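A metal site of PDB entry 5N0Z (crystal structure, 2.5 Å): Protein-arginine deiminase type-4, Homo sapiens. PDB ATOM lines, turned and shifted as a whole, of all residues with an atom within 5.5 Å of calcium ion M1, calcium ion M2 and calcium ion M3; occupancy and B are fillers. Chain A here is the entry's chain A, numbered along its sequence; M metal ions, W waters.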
ATOM      1  N   ASN A 160      -1.973 -21.280 -20.579  1.00  0.00           N
ATOM      2  CA  ASN A 160      -1.932 -21.507 -22.013  1.00  0.00           C
ATOM      3  C   ASN A 160      -1.028 -22.701 -22.325  1.00  0.00           C
ATOM      4  O   ASN A 160       0.012 -22.582 -22.929  1.00  0.00           O
ATOM      5  CB  ASN A 160      -1.477 -20.216 -22.709  1.00  0.00           C
ATOM      6  CG  ASN A 160      -1.699 -20.241 -24.191  1.00  0.00           C
ATOM      7  OD1 ASN A 160      -2.664 -20.829 -24.665  1.00  0.00           O
ATOM      8  ND2 ASN A 160      -0.814 -19.581 -24.929  1.00  0.00           N
ATOM      9  N   ASP A 162      -1.874 -25.670 -23.915  1.00  0.00           N
ATOM     10  CA  ASP A 162      -2.110 -26.448 -25.150  1.00  0.00           C
ATOM     11  C   ASP A 162      -1.072 -26.124 -26.239  1.00  0.00           C
ATOM     12  O   ASP A 162      -0.203 -25.260 -26.070  1.00  0.00           O
ATOM     13  CB  ASP A 162      -3.582 -26.319 -25.657  1.00  0.00           C
ATOM     14  CG  ASP A 162      -3.913 -24.937 -26.225  1.00  0.00           C
ATOM     15  OD1 ASP A 162      -3.017 -24.058 -26.218  1.00  0.00           O
ATOM     16  OD2 ASP A 162      -5.081 -24.695 -26.651  1.00  0.00           O
ATOM     17  N   ARG A 163      -1.193 -26.844 -27.351  1.00  0.00           N
ATOM     18  CA  ARG A 163      -0.358 -26.663 -28.555  1.00  0.00           C
ATOM     19  C   ARG A 163      -1.295 -26.370 -29.710  1.00  0.00           C
ATOM     20  O   ARG A 163      -1.842 -27.286 -30.342  1.00  0.00           O
ATOM     21  CB  ARG A 163       0.427 -27.946 -28.783  1.00  0.00           C
ATOM     22  CG  ARG A 163       1.606 -27.868 -29.721  1.00  0.00           C
ATOM     23  CD  ARG A 163       2.500 -29.065 -29.442  1.00  0.00           C
ATOM     24  NE  ARG A 163       1.875 -30.354 -29.740  1.00  0.00           N
ATOM     25  CZ  ARG A 163       2.314 -31.563 -29.336  1.00  0.00           C
ATOM     26  NH1 ARG A 163       3.422 -31.704 -28.593  1.00  0.00           N
ATOM     27  NH2 ARG A 163       1.632 -32.645 -29.664  1.00  0.00           N
ATOM     28  N   ASP A 164      -1.556 -25.078 -29.925  1.00  0.00           N
ATOM     29  CA  ASP A 164      -2.276 -24.579 -31.108  1.00  0.00           C
ATOM     30  C   ASP A 164      -1.302 -24.489 -32.276  1.00  0.00           C
ATOM     31  O   ASP A 164      -1.668 -24.728 -33.439  1.00  0.00           O
ATOM     32  CB  ASP A 164      -2.902 -23.202 -30.853  1.00  0.00           C
ATOM     33  CG  ASP A 164      -4.202 -23.283 -30.107  1.00  0.00           C
ATOM     34  OD1 ASP A 164      -4.974 -24.223 -30.312  1.00  0.00           O
ATOM     35  OD2 ASP A 164      -4.492 -22.367 -29.317  1.00  0.00           O
ATOM     36  N   ASP A 172       2.266 -23.615 -25.968  1.00  0.00           N
ATOM     37  CA  ASP A 172       2.239 -22.241 -26.473  1.00  0.00           C
ATOM     38  C   ASP A 172       2.973 -21.219 -25.606  1.00  0.00           C
ATOM     39  O   ASP A 172       3.671 -20.354 -26.144  1.00  0.00           O
ATOM     40  CB  ASP A 172       0.785 -21.771 -26.616  1.00  0.00           C
ATOM     41  CG  ASP A 172       0.028 -22.521 -27.664  1.00  0.00           C
ATOM     42  OD1 ASP A 172       0.653 -23.260 -28.465  1.00  0.00           O
ATOM     43  OD2 ASP A 172      -1.207 -22.387 -27.701  1.00  0.00           O
ATOM     44  N   CYS A 173       2.800 -21.330 -24.294  1.00  0.00           N
ATOM     45  CA  CYS A 173       3.246 -20.337 -23.314  1.00  0.00           C
ATOM     46  C   CYS A 173       4.730 -20.426 -22.903  1.00  0.00           C
ATOM     47  O   CYS A 173       5.214 -19.571 -22.141  1.00  0.00           O
ATOM     48  CB  CYS A 173       2.328 -20.389 -22.081  1.00  0.00           C
ATOM     49  SG  CYS A 173       2.364 -21.919 -21.081  1.00  0.00           S
ATOM     50  N   GLU A 174       5.464 -21.440 -23.394  1.00  0.00           N
ATOM     51  CA  GLU A 174       6.898 -21.562 -23.039  1.00  0.00           C
ATOM     52  C   GLU A 174       7.816 -20.537 -23.716  1.00  0.00           C
ATOM     53  O   GLU A 174       8.900 -20.277 -23.211  1.00  0.00           O
ATOM     54  CB  GLU A 174       7.404 -23.004 -23.231  1.00  0.00           C
ATOM     55  CG  GLU A 174       7.276 -23.867 -21.986  1.00  0.00           C
ATOM     56  CD  GLU A 174       7.030 -25.351 -22.256  1.00  0.00           C
ATOM     57  OE1 GLU A 174       7.396 -25.864 -23.346  1.00  0.00           O
ATOM     58  OE2 GLU A 174       6.499 -26.040 -21.352  1.00  0.00           O
ATOM     59  N   ASP A 175       7.396 -19.929 -24.827  1.00  0.00           N
ATOM     60  CA  ASP A 175       8.228 -18.959 -25.546  1.00  0.00           C
ATOM     61  C   ASP A 175       7.652 -17.561 -25.325  1.00  0.00           C
ATOM     62  O   ASP A 175       6.686 -17.413 -24.577  1.00  0.00           O
ATOM     63  CB  ASP A 175       8.245 -19.297 -27.049  1.00  0.00           C
ATOM     64  CG  ASP A 175       6.862 -19.120 -27.727  1.00  0.00           C
ATOM     65  OD1 ASP A 175       5.895 -18.634 -27.093  1.00  0.00           O
ATOM     66  OD2 ASP A 175       6.722 -19.491 -28.915  1.00  0.00           O
ATOM     67  N   ASP A 176       8.212 -16.556 -26.003  1.00  0.00           N
ATOM     68  CA  ASP A 176       7.769 -15.153 -25.848  1.00  0.00           C
ATOM     69  C   ASP A 176       6.841 -14.571 -26.944  1.00  0.00           C
ATOM     70  O   ASP A 176       6.616 -13.349 -26.955  1.00  0.00           O
ATOM     71  CB  ASP A 176       9.014 -14.251 -25.706  1.00  0.00           C
ATOM     72  CG  ASP A 176       9.688 -14.372 -24.348  1.00  0.00           C
ATOM     73  OD1 ASP A 176       9.001 -14.531 -23.308  1.00  0.00           O
ATOM     74  OD2 ASP A 176      10.937 -14.273 -24.315  1.00  0.00           O
ATOM     75  N   GLU A 177       6.276 -15.410 -27.830  1.00  0.00           N
ATOM     76  CA  GLU A 177       5.520 -14.939 -29.031  1.00  0.00           C
ATOM     77  C   GLU A 177       4.122 -15.554 -29.204  1.00  0.00           C
ATOM     78  O   GLU A 177       3.900 -16.718 -28.842  1.00  0.00           O
ATOM     79  CB  GLU A 177       6.298 -15.248 -30.322  1.00  0.00           C
ATOM     80  CG  GLU A 177       7.819 -15.254 -30.204  1.00  0.00           C
ATOM     81  CD  GLU A 177       8.515 -15.368 -31.556  1.00  0.00           C
ATOM     82  OE1 GLU A 177       8.236 -14.533 -32.453  1.00  0.00           O
ATOM     83  OE2 GLU A 177       9.354 -16.267 -31.706  1.00  0.00           O
ATOM     84  N   VAL A 178       3.197 -14.776 -29.782  1.00  0.00           N
ATOM     85  CA  VAL A 178       1.928 -15.282 -30.352  1.00  0.00           C
ATOM     86  C   VAL A 178       2.171 -15.635 -31.824  1.00  0.00           C
ATOM     87  O   VAL A 178       2.355 -14.744 -32.667  1.00  0.00           O
ATOM     88  CB  VAL A 178       0.800 -14.240 -30.307  1.00  0.00           C
ATOM     89  CG1 VAL A 178      -0.440 -14.744 -31.022  1.00  0.00           C
ATOM     90  CG2 VAL A 178       0.447 -13.866 -28.888  1.00  0.00           C
ATOM     91  N   LEU A 179       2.130 -16.924 -32.148  1.00  0.00           N
ATOM     92  CA  LEU A 179       2.446 -17.383 -33.500  1.00  0.00           C
ATOM     93  C   LEU A 179       1.197 -17.600 -34.339  1.00  0.00           C
ATOM     94  O   LEU A 179       1.189 -17.268 -35.509  1.00  0.00           O
ATOM     95  CB  LEU A 179       3.303 -18.641 -33.439  1.00  0.00           C
ATOM     96  CG  LEU A 179       4.647 -18.406 -32.760  1.00  0.00           C
ATOM     97  CD1 LEU A 179       5.347 -19.728 -32.489  1.00  0.00           C
ATOM     98  CD2 LEU A 179       5.553 -17.465 -33.561  1.00  0.00           C
ATOM     99  N   GLU A 182      -5.273 -18.065 -33.565  1.00  0.00           N
ATOM    100  CA  GLU A 182      -6.086 -18.997 -32.788  1.00  0.00           C
ATOM    101  C   GLU A 182      -5.702 -18.931 -31.317  1.00  0.00           C
ATOM    102  O   GLU A 182      -6.565 -18.963 -30.429  1.00  0.00           O
ATOM    103  CB  GLU A 182      -5.899 -20.460 -33.261  1.00  0.00           C
ATOM    104  CG  GLU A 182      -6.662 -20.879 -34.526  1.00  0.00           C
ATOM    105  CD  GLU A 182      -6.002 -20.436 -35.836  1.00  0.00           C
ATOM    106  OE1 GLU A 182      -6.770 -20.181 -36.779  1.00  0.00           O
ATOM    107  OE2 GLU A 182      -4.745 -20.328 -35.918  1.00  0.00           O
ATOM    108  N   ASP A 183      -4.384 -18.856 -31.091  1.00  0.00           N
ATOM    109  CA  ASP A 183      -3.785 -18.764 -29.757  1.00  0.00           C
ATOM    110  C   ASP A 183      -4.438 -17.675 -28.897  1.00  0.00           C
ATOM    111  O   ASP A 183      -4.721 -17.901 -27.708  1.00  0.00           O
ATOM    112  CB  ASP A 183      -2.253 -18.542 -29.877  1.00  0.00           C
ATOM    113  CG  ASP A 183      -1.490 -18.888 -28.604  1.00  0.00           C
ATOM    114  OD1 ASP A 183      -2.006 -19.692 -27.810  1.00  0.00           O
ATOM    115  OD2 ASP A 183      -0.343 -18.377 -28.433  1.00  0.00           O
ATOM    116  N   ASP A 186      -7.359 -18.352 -26.461  1.00  0.00           N
ATOM    117  CA  ASP A 186      -7.054 -18.883 -25.140  1.00  0.00           C
ATOM    118  C   ASP A 186      -6.749 -17.791 -24.114  1.00  0.00           C
ATOM    119  O   ASP A 186      -6.941 -17.988 -22.909  1.00  0.00           O
ATOM    120  CB  ASP A 186      -5.889 -19.891 -25.240  1.00  0.00           C
ATOM    121  CG  ASP A 186      -6.250 -21.111 -26.088  1.00  0.00           C
ATOM    122  OD1 ASP A 186      -7.461 -21.485 -26.183  1.00  0.00           O
ATOM    123  OD2 ASP A 186      -5.306 -21.696 -26.703  1.00  0.00           O
ATOM    124  N   PHE A 221       0.760  -9.513 -23.810  1.00  0.00           N
ATOM    125  CA  PHE A 221       1.062  -9.017 -25.153  1.00  0.00           C
ATOM    126  C   PHE A 221       0.277  -7.769 -25.482  1.00  0.00           C
ATOM    127  O   PHE A 221      -0.922  -7.673 -25.184  1.00  0.00           O
ATOM    128  CB  PHE A 221       0.696 -10.072 -26.167  1.00  0.00           C
ATOM    129  CG  PHE A 221       1.458 -11.341 -26.020  1.00  0.00           C
ATOM    130  CD1 PHE A 221       2.716 -11.471 -26.569  1.00  0.00           C
ATOM    131  CD2 PHE A 221       0.891 -12.428 -25.350  1.00  0.00           C
ATOM    132  CE1 PHE A 221       3.419 -12.654 -26.445  1.00  0.00           C
ATOM    133  CE2 PHE A 221       1.590 -13.623 -25.230  1.00  0.00           C
ATOM    134  CZ  PHE A 221       2.853 -13.741 -25.775  1.00  0.00           C
ATOM    135  N   GLU A 259      -1.820 -14.422 -20.875  1.00  0.00           N
ATOM    136  CA  GLU A 259      -1.796 -15.850 -20.654  1.00  0.00           C
ATOM    137  C   GLU A 259      -1.091 -16.075 -19.337  1.00  0.00           C
ATOM    138  O   GLU A 259      -0.174 -15.355 -18.994  1.00  0.00           O
ATOM    139  CB  GLU A 259      -1.048 -16.607 -21.791  1.00  0.00           C
ATOM    140  CG  GLU A 259       0.286 -15.963 -22.197  1.00  0.00           C
ATOM    141  CD  GLU A 259       1.162 -16.767 -23.171  1.00  0.00           C
ATOM    142  OE1 GLU A 259       0.634 -17.463 -24.077  1.00  0.00           O
ATOM    143  OE2 GLU A 259       2.417 -16.675 -23.018  1.00  0.00           O
ATOM    144  N   LYS A 369     -13.383 -19.290 -22.860  1.00  0.00           N
ATOM    145  CA  LYS A 369     -12.698 -20.463 -23.387  1.00  0.00           C
ATOM    146  C   LYS A 369     -12.703 -21.598 -22.377  1.00  0.00           C
ATOM    147  O   LYS A 369     -12.571 -21.387 -21.198  1.00  0.00           O
ATOM    148  CB  LYS A 369     -11.264 -20.137 -23.794  1.00  0.00           C
ATOM    149  CG  LYS A 369     -10.457 -21.327 -24.300  1.00  0.00           C
ATOM    150  CD  LYS A 369     -11.068 -22.031 -25.510  1.00  0.00           C
ATOM    151  CE  LYS A 369     -10.920 -21.264 -26.805  1.00  0.00           C
ATOM    152  NZ  LYS A 369     -11.051 -22.192 -27.951  1.00  0.00           N
ATOM    153  N   LEU A 371     -11.254 -25.724 -22.270  1.00  0.00           N
ATOM    154  CA  LEU A 371     -10.565 -26.691 -23.035  1.00  0.00           C
ATOM    155  C   LEU A 371     -10.017 -27.801 -22.166  1.00  0.00           C
ATOM    156  O   LEU A 371      -9.589 -27.568 -21.041  1.00  0.00           O
ATOM    157  CB  LEU A 371      -9.489 -26.006 -23.850  1.00  0.00           C
ATOM    158  CG  LEU A 371      -8.367 -25.311 -23.104  1.00  0.00           C
ATOM    159  CD1 LEU A 371      -7.193 -26.269 -22.993  1.00  0.00           C
ATOM    160  CD2 LEU A 371      -7.843 -24.072 -23.774  1.00  0.00           C
ATOM    161  N   PRO A 394      -4.125 -29.034 -30.486  1.00  0.00           N
ATOM    162  CA  PRO A 394      -5.025 -27.913 -30.716  1.00  0.00           C
ATOM    163  C   PRO A 394      -6.241 -27.976 -29.803  1.00  0.00           C
ATOM    164  O   PRO A 394      -7.050 -28.890 -29.943  1.00  0.00           O
ATOM    165  CB  PRO A 394      -5.432 -28.089 -32.187  1.00  0.00           C
ATOM    166  CG  PRO A 394      -4.255 -28.766 -32.811  1.00  0.00           C
ATOM    167  CD  PRO A 394      -3.635 -29.631 -31.752  1.00  0.00           C
ATOM    168  N   ASP A 395      -6.358 -27.038 -28.878  1.00  0.00           N
ATOM    169  CA  ASP A 395      -7.423 -27.053 -27.854  1.00  0.00           C
ATOM    170  C   ASP A 395      -7.362 -28.308 -26.929  1.00  0.00           C
ATOM    171  O   ASP A 395      -8.392 -28.836 -26.481  1.00  0.00           O
ATOM    172  CB  ASP A 395      -8.821 -26.856 -28.498  1.00  0.00           C
ATOM    173  CG  ASP A 395      -9.104 -25.418 -28.875  1.00  0.00           C
ATOM    174  OD1 ASP A 395      -8.173 -24.597 -28.907  1.00  0.00           O
ATOM    175  OD2 ASP A 395     -10.281 -25.097 -29.106  1.00  0.00           O
HETATM  176 CA    CA M   1      -6.471 -23.348 -27.919  1.00  0.00          CA
HETATM  177 CA    CA M   2      -3.052 -21.795 -26.997  1.00  0.00          CA
HETATM  178 CA    CA M   3       3.504 -18.512 -27.519  1.00  0.00          CA
HETATM  179  O   HOH W   1       4.038 -20.290 -29.185  1.00  0.00           O
HETATM  180  O   HOH W   2       4.169 -17.185 -25.539  1.00  0.00           O
HETATM  181  O   HOH W   3      -7.203 -21.656 -29.402  1.00  0.00           O
HETATM  182  O   HOH W   4       1.655 -17.962 -26.855  1.00  0.00           O
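The side-chain carboxylate (OE1) of Glu 259 sits at hydrogen-bond distance from the side-chain amide nitrogen (ND2) of Asn 160 (2.7 Å). The side-chain carboxylate (OD2) of Asp 395 lies within salt-bridge range of the side-chain amino group (NZ) of Lys 369, at 3.2 Å. The backbone carbonyl oxygen (O) of Asn 160 lies within hydrogen-bond range of the side-chain sulfur (SG) of Cys 173 (3.1 Å).
Calcium ion M3 is bound by water W4 (2.0 Å), O of Glu 177 (2.3 Å), O of Asp 172 (2.3 Å), OD1 of Asp 175 (2.4 Å), water W2 (2.5 Å) and water W1 (2.5 Å). Calcium ion M3 has six donor atoms within binding distance.
Of the 21 residues printed, 4 come within 4 Å of calcium ion M3.
Calcium ion M2 is bound by the side-chain carboxylate of Asp 172 (2.1 Å), the side-chain carboxylate of Asp 186 (2.3 Å), the side-chain carboxylate of Asp 162 (2.4 Å), the side-chain carboxylate of Asp 183 (2.5 Å), the side-chain amide oxygen of Asn 160 (2.6 Å) and the side-chain carboxylate of Asp 164 (2.8 Å). Calcium ion M2 has six donor atoms within binding distance.
Water W2 lies within hydrogen-bond range of the backbone carbonyl oxygen (O) of Asp 175 (2.7 Å) and the side-chain carboxylate (OE2) of Glu 259 (3.1 Å). Water W4 lies within hydrogen-bond range of OD2 of Asp 183 (2.6 Å) and OE1 of Glu 259 (3.0 Å).
Six residues have an atom within 4 Å of calcium ion M2: Asn 160, Asp 162, Asp 164, Asp 172, Asp 183 and Asp 186. The nearest printed residue that does not touch calcium ion M2 is Arg 163 (5.4 Å).
Calcium ion M1 is bound by the side-chain carboxylate (OD2) of Asp 162, the side-chain carboxylate (OD1) of Asp 395, the side-chain carboxylate (OD2) of Asp 186, water W3, the side-chain carboxylate (OD2) of Asp 164 and the side-chain carboxylate (OD1) of Asp 186. Calcium ion M1 has six donor atoms within binding distance. Slightly farther from calcium ion M1 lies the side-chain carboxylate (OD1) of Asp 164 (3.0 Å).
Of the 21 residues printed, 4 come within 4 Å of calcium ion M1.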
